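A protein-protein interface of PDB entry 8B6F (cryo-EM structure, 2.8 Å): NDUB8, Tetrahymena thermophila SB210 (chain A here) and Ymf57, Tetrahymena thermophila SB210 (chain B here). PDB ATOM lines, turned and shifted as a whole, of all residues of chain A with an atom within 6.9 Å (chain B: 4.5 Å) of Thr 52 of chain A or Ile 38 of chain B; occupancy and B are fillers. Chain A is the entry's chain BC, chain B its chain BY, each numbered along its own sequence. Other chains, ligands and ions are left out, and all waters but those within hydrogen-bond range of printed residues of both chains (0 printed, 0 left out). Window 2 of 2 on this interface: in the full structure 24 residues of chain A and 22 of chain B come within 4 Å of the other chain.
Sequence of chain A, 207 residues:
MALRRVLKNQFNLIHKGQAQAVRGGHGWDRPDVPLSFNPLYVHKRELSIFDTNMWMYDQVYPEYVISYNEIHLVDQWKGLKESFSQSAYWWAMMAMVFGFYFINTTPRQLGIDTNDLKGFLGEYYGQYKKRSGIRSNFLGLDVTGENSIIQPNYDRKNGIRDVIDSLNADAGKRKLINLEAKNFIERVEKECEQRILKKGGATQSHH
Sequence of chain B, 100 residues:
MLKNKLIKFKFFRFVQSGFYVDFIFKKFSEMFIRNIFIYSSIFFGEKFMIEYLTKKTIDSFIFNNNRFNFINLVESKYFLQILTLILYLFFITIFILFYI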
ATOM      1  N   LEU A  47      10.172 -33.487  17.638  1.00  0.00           N
ATOM      2  CA  LEU A  47      10.184 -32.523  18.735  1.00  0.00           C
ATOM      3  C   LEU A  47       8.741 -32.118  18.998  1.00  0.00           C
ATOM      4  O   LEU A  47       8.198 -31.235  18.333  1.00  0.00           O
ATOM      5  CB  LEU A  47      11.054 -31.318  18.393  1.00  0.00           C
ATOM      6  CG  LEU A  47      12.550 -31.559  18.140  1.00  0.00           C
ATOM      7  CD1 LEU A  47      12.810 -32.201  16.785  1.00  0.00           C
ATOM      8  CD2 LEU A  47      13.333 -30.265  18.266  1.00  0.00           C
ATOM      9  N   SER A  48       8.112 -32.778  19.964  1.00  0.00           N
ATOM     10  CA  SER A  48       6.710 -32.518  20.251  1.00  0.00           C
ATOM     11  C   SER A  48       6.513 -31.086  20.726  1.00  0.00           C
ATOM     12  O   SER A  48       7.305 -30.556  21.508  1.00  0.00           O
ATOM     13  CB  SER A  48       6.202 -33.497  21.308  1.00  0.00           C
ATOM     14  OG  SER A  48       4.879 -33.181  21.704  1.00  0.00           O
ATOM     15  N   ILE A  49       5.445 -30.453  20.235  1.00  0.00           N
ATOM     16  CA  ILE A  49       5.108 -29.110  20.686  1.00  0.00           C
ATOM     17  C   ILE A  49       4.670 -29.111  22.141  1.00  0.00           C
ATOM     18  O   ILE A  49       4.687 -28.060  22.790  1.00  0.00           O
ATOM     19  CB  ILE A  49       4.015 -28.491  19.795  1.00  0.00           C
ATOM     20  CG1 ILE A  49       2.773 -29.388  19.771  1.00  0.00           C
ATOM     21  CG2 ILE A  49       4.556 -28.266  18.392  1.00  0.00           C
ATOM     22  CD1 ILE A  49       1.602 -28.794  19.030  1.00  0.00           C
ATOM     23  N   PHE A  50       4.264 -30.266  22.671  1.00  0.00           N
ATOM     24  CA  PHE A  50       3.908 -30.370  24.079  1.00  0.00           C
ATOM     25  C   PHE A  50       5.126 -30.363  24.991  1.00  0.00           C
ATOM     26  O   PHE A  50       4.961 -30.278  26.212  1.00  0.00           O
ATOM     27  CB  PHE A  50       3.086 -31.635  24.320  1.00  0.00           C
ATOM     28  CG  PHE A  50       1.831 -31.705  23.501  1.00  0.00           C
ATOM     29  CD1 PHE A  50       0.715 -30.967  23.859  1.00  0.00           C
ATOM     30  CD2 PHE A  50       1.764 -32.513  22.379  1.00  0.00           C
ATOM     31  CE1 PHE A  50      -0.443 -31.030  23.109  1.00  0.00           C
ATOM     32  CE2 PHE A  50       0.609 -32.579  21.625  1.00  0.00           C
ATOM     33  CZ  PHE A  50      -0.497 -31.835  21.991  1.00  0.00           C
ATOM     34  N   ASP A  51       6.333 -30.463  24.433  1.00  0.00           N
ATOM     35  CA  ASP A  51       7.574 -30.358  25.192  1.00  0.00           C
ATOM     36  C   ASP A  51       8.319 -29.064  24.893  1.00  0.00           C
ATOM     37  O   ASP A  51       9.536 -28.995  25.087  1.00  0.00           O
ATOM     38  CB  ASP A  51       8.477 -31.556  24.902  1.00  0.00           C
ATOM     39  CG  ASP A  51       7.910 -32.856  25.425  1.00  0.00           C
ATOM     40  OD1 ASP A  51       7.244 -32.830  26.480  1.00  0.00           O
ATOM     41  OD2 ASP A  51       8.133 -33.904  24.788  1.00  0.00           O
ATOM     42  N   THR A  52       7.618 -28.037  24.418  1.00  0.00           N
ATOM     43  CA  THR A  52       8.277 -26.792  24.054  1.00  0.00           C
ATOM     44  C   THR A  52       9.016 -26.216  25.255  1.00  0.00           C
ATOM     45  O   THR A  52       8.455 -26.096  26.347  1.00  0.00           O
ATOM     46  CB  THR A  52       7.255 -25.787  23.518  1.00  0.00           C
ATOM     47  OG1 THR A  52       7.920 -24.575  23.139  1.00  0.00           O
ATOM     48  CG2 THR A  52       6.188 -25.477  24.564  1.00  0.00           C
ATOM     49  N   ASN A  53      10.284 -25.873  25.051  1.00  0.00           N
ATOM     50  CA  ASN A  53      11.159 -25.328  26.083  1.00  0.00           C
ATOM     51  C   ASN A  53      11.349 -26.277  27.260  1.00  0.00           C
ATOM     52  O   ASN A  53      11.892 -25.871  28.294  1.00  0.00           O
ATOM     53  CB  ASN A  53      10.651 -23.970  26.588  1.00  0.00           C
ATOM     54  CG  ASN A  53      11.086 -22.819  25.703  1.00  0.00           C
ATOM     55  OD1 ASN A  53      11.603 -23.026  24.607  1.00  0.00           O
ATOM     56  ND2 ASN A  53      10.874 -21.598  26.174  1.00  0.00           N
ATOM     57  N   MET A  54      10.915 -27.531  27.139  1.00  0.00           N
ATOM     58  CA  MET A  54      11.211 -28.543  28.143  1.00  0.00           C
ATOM     59  C   MET A  54      12.517 -29.270  27.867  1.00  0.00           C
ATOM     60  O   MET A  54      12.957 -30.062  28.706  1.00  0.00           O
ATOM     61  CB  MET A  54      10.073 -29.564  28.232  1.00  0.00           C
ATOM     62  CG  MET A  54       8.762 -28.995  28.754  1.00  0.00           C
ATOM     63  SD  MET A  54       8.897 -28.273  30.401  1.00  0.00           S
ATOM     64  CE  MET A  54       9.446 -29.677  31.366  1.00  0.00           C
ATOM     65  N   TRP A  55      13.137 -29.027  26.715  1.00  0.00           N
ATOM     66  CA  TRP A  55      14.446 -29.565  26.379  1.00  0.00           C
ATOM     67  C   TRP A  55      15.416 -28.410  26.188  1.00  0.00           C
ATOM     68  O   TRP A  55      15.102 -27.446  25.484  1.00  0.00           O
ATOM     69  CB  TRP A  55      14.387 -30.417  25.111  1.00  0.00           C
ATOM     70  CG  TRP A  55      13.610 -31.676  25.274  1.00  0.00           C
ATOM     71  CD1 TRP A  55      12.265 -31.835  25.123  1.00  0.00           C
ATOM     72  CD2 TRP A  55      14.130 -32.963  25.620  1.00  0.00           C
ATOM     73  NE1 TRP A  55      11.916 -33.142  25.357  1.00  0.00           N
ATOM     74  CE2 TRP A  55      13.043 -33.855  25.663  1.00  0.00           C
ATOM     75  CE3 TRP A  55      15.412 -33.446  25.900  1.00  0.00           C
ATOM     76  CZ2 TRP A  55      13.197 -35.202  25.975  1.00  0.00           C
ATOM     77  CZ3 TRP A  55      15.563 -34.783  26.207  1.00  0.00           C
ATOM     78  CH2 TRP A  55      14.463 -35.647  26.243  1.00  0.00           C
ATOM     79  N   TYR A  57      17.770 -27.179  24.230  1.00  0.00           N
ATOM     80  CA  TYR A  57      18.159 -27.531  22.872  1.00  0.00           C
ATOM     81  C   TYR A  57      19.637 -27.255  22.641  1.00  0.00           C
ATOM     82  O   TYR A  57      20.174 -26.233  23.076  1.00  0.00           O
ATOM     83  CB  TYR A  57      17.316 -26.749  21.864  1.00  0.00           C
ATOM     84  CG  TYR A  57      15.833 -27.001  21.998  1.00  0.00           C
ATOM     85  CD1 TYR A  57      15.250 -28.134  21.450  1.00  0.00           C
ATOM     86  CD2 TYR A  57      15.016 -26.103  22.668  1.00  0.00           C
ATOM     87  CE1 TYR A  57      13.896 -28.369  21.572  1.00  0.00           C
ATOM     88  CE2 TYR A  57      13.662 -26.328  22.794  1.00  0.00           C
ATOM     89  CZ  TYR A  57      13.107 -27.462  22.243  1.00  0.00           C
ATOM     90  OH  TYR A  57      11.758 -27.691  22.365  1.00  0.00           O
ATOM     91  N   ILE B  33       5.647 -26.422  35.698  1.00  0.00           N
ATOM     92  CA  ILE B  33       6.016 -25.900  34.384  1.00  0.00           C
ATOM     93  C   ILE B  33       5.122 -26.494  33.304  1.00  0.00           C
ATOM     94  O   ILE B  33       4.547 -25.771  32.484  1.00  0.00           O
ATOM     95  CB  ILE B  33       7.502 -26.185  34.094  1.00  0.00           C
ATOM     96  CG1 ILE B  33       8.395 -25.364  35.024  1.00  0.00           C
ATOM     97  CG2 ILE B  33       7.843 -25.881  32.637  1.00  0.00           C
ATOM     98  CD1 ILE B  33       9.839 -25.818  35.030  1.00  0.00           C
ATOM     99  N   ARG B  34       4.983 -27.818  33.294  1.00  0.00           N
ATOM    100  CA  ARG B  34       4.205 -28.459  32.239  1.00  0.00           C
ATOM    101  C   ARG B  34       2.748 -28.026  32.281  1.00  0.00           C
ATOM    102  O   ARG B  34       2.145 -27.753  31.237  1.00  0.00           O
ATOM    103  CB  ARG B  34       4.313 -29.977  32.360  1.00  0.00           C
ATOM    104  CG  ARG B  34       5.722 -30.511  32.173  1.00  0.00           C
ATOM    105  CD  ARG B  34       5.710 -32.001  31.899  1.00  0.00           C
ATOM    106  NE  ARG B  34       5.229 -32.285  30.554  1.00  0.00           N
ATOM    107  CZ  ARG B  34       5.996 -32.325  29.475  1.00  0.00           C
ATOM    108  NH1 ARG B  34       7.304 -32.146  29.546  1.00  0.00           N
ATOM    109  NH2 ARG B  34       5.434 -32.541  28.290  1.00  0.00           N
ATOM    110  N   ILE B  36       1.316 -25.291  33.734  1.00  0.00           N
ATOM    111  CA  ILE B  36       1.003 -23.867  33.679  1.00  0.00           C
ATOM    112  C   ILE B  36       1.527 -23.228  32.399  1.00  0.00           C
ATOM    113  O   ILE B  36       0.841 -22.406  31.789  1.00  0.00           O
ATOM    114  CB  ILE B  36       1.562 -23.162  34.930  1.00  0.00           C
ATOM    115  CG1 ILE B  36       0.979 -23.780  36.209  1.00  0.00           C
ATOM    116  CG2 ILE B  36       1.277 -21.664  34.884  1.00  0.00           C
ATOM    117  CD1 ILE B  36      -0.532 -23.700  36.319  1.00  0.00           C
ATOM    118  N   PHE B  37       2.741 -23.579  31.975  1.00  0.00           N
ATOM    119  CA  PHE B  37       3.371 -22.893  30.857  1.00  0.00           C
ATOM    120  C   PHE B  37       3.009 -23.471  29.497  1.00  0.00           C
ATOM    121  O   PHE B  37       3.289 -22.823  28.484  1.00  0.00           O
ATOM    122  CB  PHE B  37       4.897 -22.915  31.010  1.00  0.00           C
ATOM    123  CG  PHE B  37       5.415 -22.093  32.163  1.00  0.00           C
ATOM    124  CD1 PHE B  37       4.646 -21.092  32.735  1.00  0.00           C
ATOM    125  CD2 PHE B  37       6.685 -22.319  32.663  1.00  0.00           C
ATOM    126  CE1 PHE B  37       5.134 -20.341  33.783  1.00  0.00           C
ATOM    127  CE2 PHE B  37       7.177 -21.571  33.712  1.00  0.00           C
ATOM    128  CZ  PHE B  37       6.401 -20.582  34.272  1.00  0.00           C
ATOM    129  N   ILE B  38       2.398 -24.654  29.438  1.00  0.00           N
ATOM    130  CA  ILE B  38       2.131 -25.292  28.152  1.00  0.00           C
ATOM    131  C   ILE B  38       0.645 -25.587  27.992  1.00  0.00           C
ATOM    132  O   ILE B  38      -0.013 -25.049  27.096  1.00  0.00           O
ATOM    133  CB  ILE B  38       2.958 -26.581  27.997  1.00  0.00           C
ATOM    134  CG1 ILE B  38       4.440 -26.288  28.239  1.00  0.00           C
ATOM    135  CG2 ILE B  38       2.748 -27.176  26.610  1.00  0.00           C
ATOM    136  CD1 ILE B  38       5.325 -27.513  28.219  1.00  0.00           C
ATOM    137  N   TYR B  39       0.108 -26.442  28.861  1.00  0.00           N
ATOM    138  CA  TYR B  39      -1.255 -26.926  28.669  1.00  0.00           C
ATOM    139  C   TYR B  39      -2.279 -25.844  28.969  1.00  0.00           C
ATOM    140  O   TYR B  39      -3.253 -25.678  28.225  1.00  0.00           O
ATOM    141  CB  TYR B  39      -1.502 -28.151  29.546  1.00  0.00           C
ATOM    142  CG  TYR B  39      -0.454 -29.226  29.392  1.00  0.00           C
ATOM    143  CD1 TYR B  39       0.189 -29.427  28.178  1.00  0.00           C
ATOM    144  CD2 TYR B  39      -0.100 -30.032  30.461  1.00  0.00           C
ATOM    145  CE1 TYR B  39       1.149 -30.403  28.033  1.00  0.00           C
ATOM    146  CE2 TYR B  39       0.861 -31.012  30.326  1.00  0.00           C
ATOM    147  CZ  TYR B  39       1.481 -31.192  29.110  1.00  0.00           C
ATOM    148  OH  TYR B  39       2.439 -32.167  28.970  1.00  0.00           O
ATOM    149  N   SER B  40      -2.079 -25.100  30.050  1.00  0.00           N
ATOM    150  CA  SER B  40      -3.046 -24.104  30.483  1.00  0.00           C
ATOM    151  C   SER B  40      -2.837 -22.758  29.806  1.00  0.00           C
ATOM    152  O   SER B  40      -3.811 -22.081  29.461  1.00  0.00           O
ATOM    153  CB  SER B  40      -2.969 -23.935  32.001  1.00  0.00           C
ATOM    154  OG  SER B  40      -3.971 -23.051  32.463  1.00  0.00           O
ATOM    155  N   SER B  41      -1.586 -22.353  29.609  1.00  0.00           N
ATOM    156  CA  SER B  41      -1.290 -21.037  29.055  1.00  0.00           C
ATOM    157  C   SER B  41      -1.267 -21.045  27.530  1.00  0.00           C
ATOM    158  O   SER B  41      -1.975 -20.263  26.889  1.00  0.00           O
ATOM    159  CB  SER B  41       0.047 -20.535  29.601  1.00  0.00           C
ATOM    160  OG  SER B  41       0.327 -19.249  29.088  1.00  0.00           O
ATOM    161  N   ILE B  42      -0.455 -21.916  26.936  1.00  0.00           N
ATOM    162  CA  ILE B  42      -0.317 -21.928  25.484  1.00  0.00           C
ATOM    163  C   ILE B  42      -1.567 -22.513  24.836  1.00  0.00           C
ATOM    164  O   ILE B  42      -2.256 -21.845  24.060  1.00  0.00           O
ATOM    165  CB  ILE B  42       0.951 -22.695  25.069  1.00  0.00           C
ATOM    166  CG1 ILE B  42       2.204 -21.979  25.581  1.00  0.00           C
ATOM    167  CG2 ILE B  42       1.010 -22.873  23.562  1.00  0.00           C
ATOM    168  CD1 ILE B  42       2.458 -20.621  24.953  1.00  0.00           C
ATOM    169  N   PHE B  43      -1.885 -23.766  25.150  1.00  0.00           N
ATOM    170  CA  PHE B  43      -2.978 -24.433  24.450  1.00  0.00           C
ATOM    171  C   PHE B  43      -4.332 -23.918  24.921  1.00  0.00           C
ATOM    172  O   PHE B  43      -5.095 -23.343  24.139  1.00  0.00           O
ATOM    173  CB  PHE B  43      -2.864 -25.945  24.628  1.00  0.00           C
ATOM    174  CG  PHE B  43      -1.690 -26.538  23.910  1.00  0.00           C
ATOM    175  CD1 PHE B  43      -1.741 -26.760  22.545  1.00  0.00           C
ATOM    176  CD2 PHE B  43      -0.531 -26.859  24.593  1.00  0.00           C
ATOM    177  CE1 PHE B  43      -0.663 -27.297  21.876  1.00  0.00           C
ATOM    178  CE2 PHE B  43       0.551 -27.397  23.929  1.00  0.00           C
ATOM    179  CZ  PHE B  43       0.485 -27.616  22.568  1.00  0.00           C
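NH2 of Arg 34 of chain B lies within salt-bridge range of OD1 of Asp 51 of chain A (2.6 Å). NH2 of Arg 34 of chain B lies within hydrogen-bond range of O of Phe 50 of chain A (3.1 Å).
The backbone carbonyl oxygen of Ile 38 of chain B is in hydrogen-bond range of the backbone NH of Phe 43 of chain B (3.0 Å). NH2 of Arg 34 of chain B sits at hydrogen-bond distance from OH of Tyr 39 of chain B (3.1 Å). OG of Ser 48 of chain A sits close to N of Phe 50 of chain A (3.1 Å).
Among the printed residues, pairs that only touch across the chains: Ile 49 of chain A with Phe 43 of chain B, Phe 50 of chain A with Ile 38 of chain B, Phe 50 of chain A with Phe 43 of chain B, Thr 52 of chain A with Ile 38 of chain B, Met 54 of chain A with Ile 33 of chain B, Met 54 of chain A with Arg 34 of chain B and Met 54 of chain A with Ile 38 of chain B.
Thr 52 of chain A touches just one residue of chain B: Ile 38. Ile 38 of chain B touches three residues of chain A. Of the printed residues of chain A, Ile 33 of chain B touches Met 54. Of the printed residues of chain B, Met 54 of chain A touches Ile 33, Arg 34 and Ile 38. Printed residues of chain B within 4 Å of Asp 51 of chain A: Arg 34 (2.6 Å).
Among the printed residues, Asp or Glu carboxylates within 4 Å of a Lys or Arg side-chain nitrogen of the other chain: Asp 51 of chain A with Arg 34 of chain B (2.6 Å).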
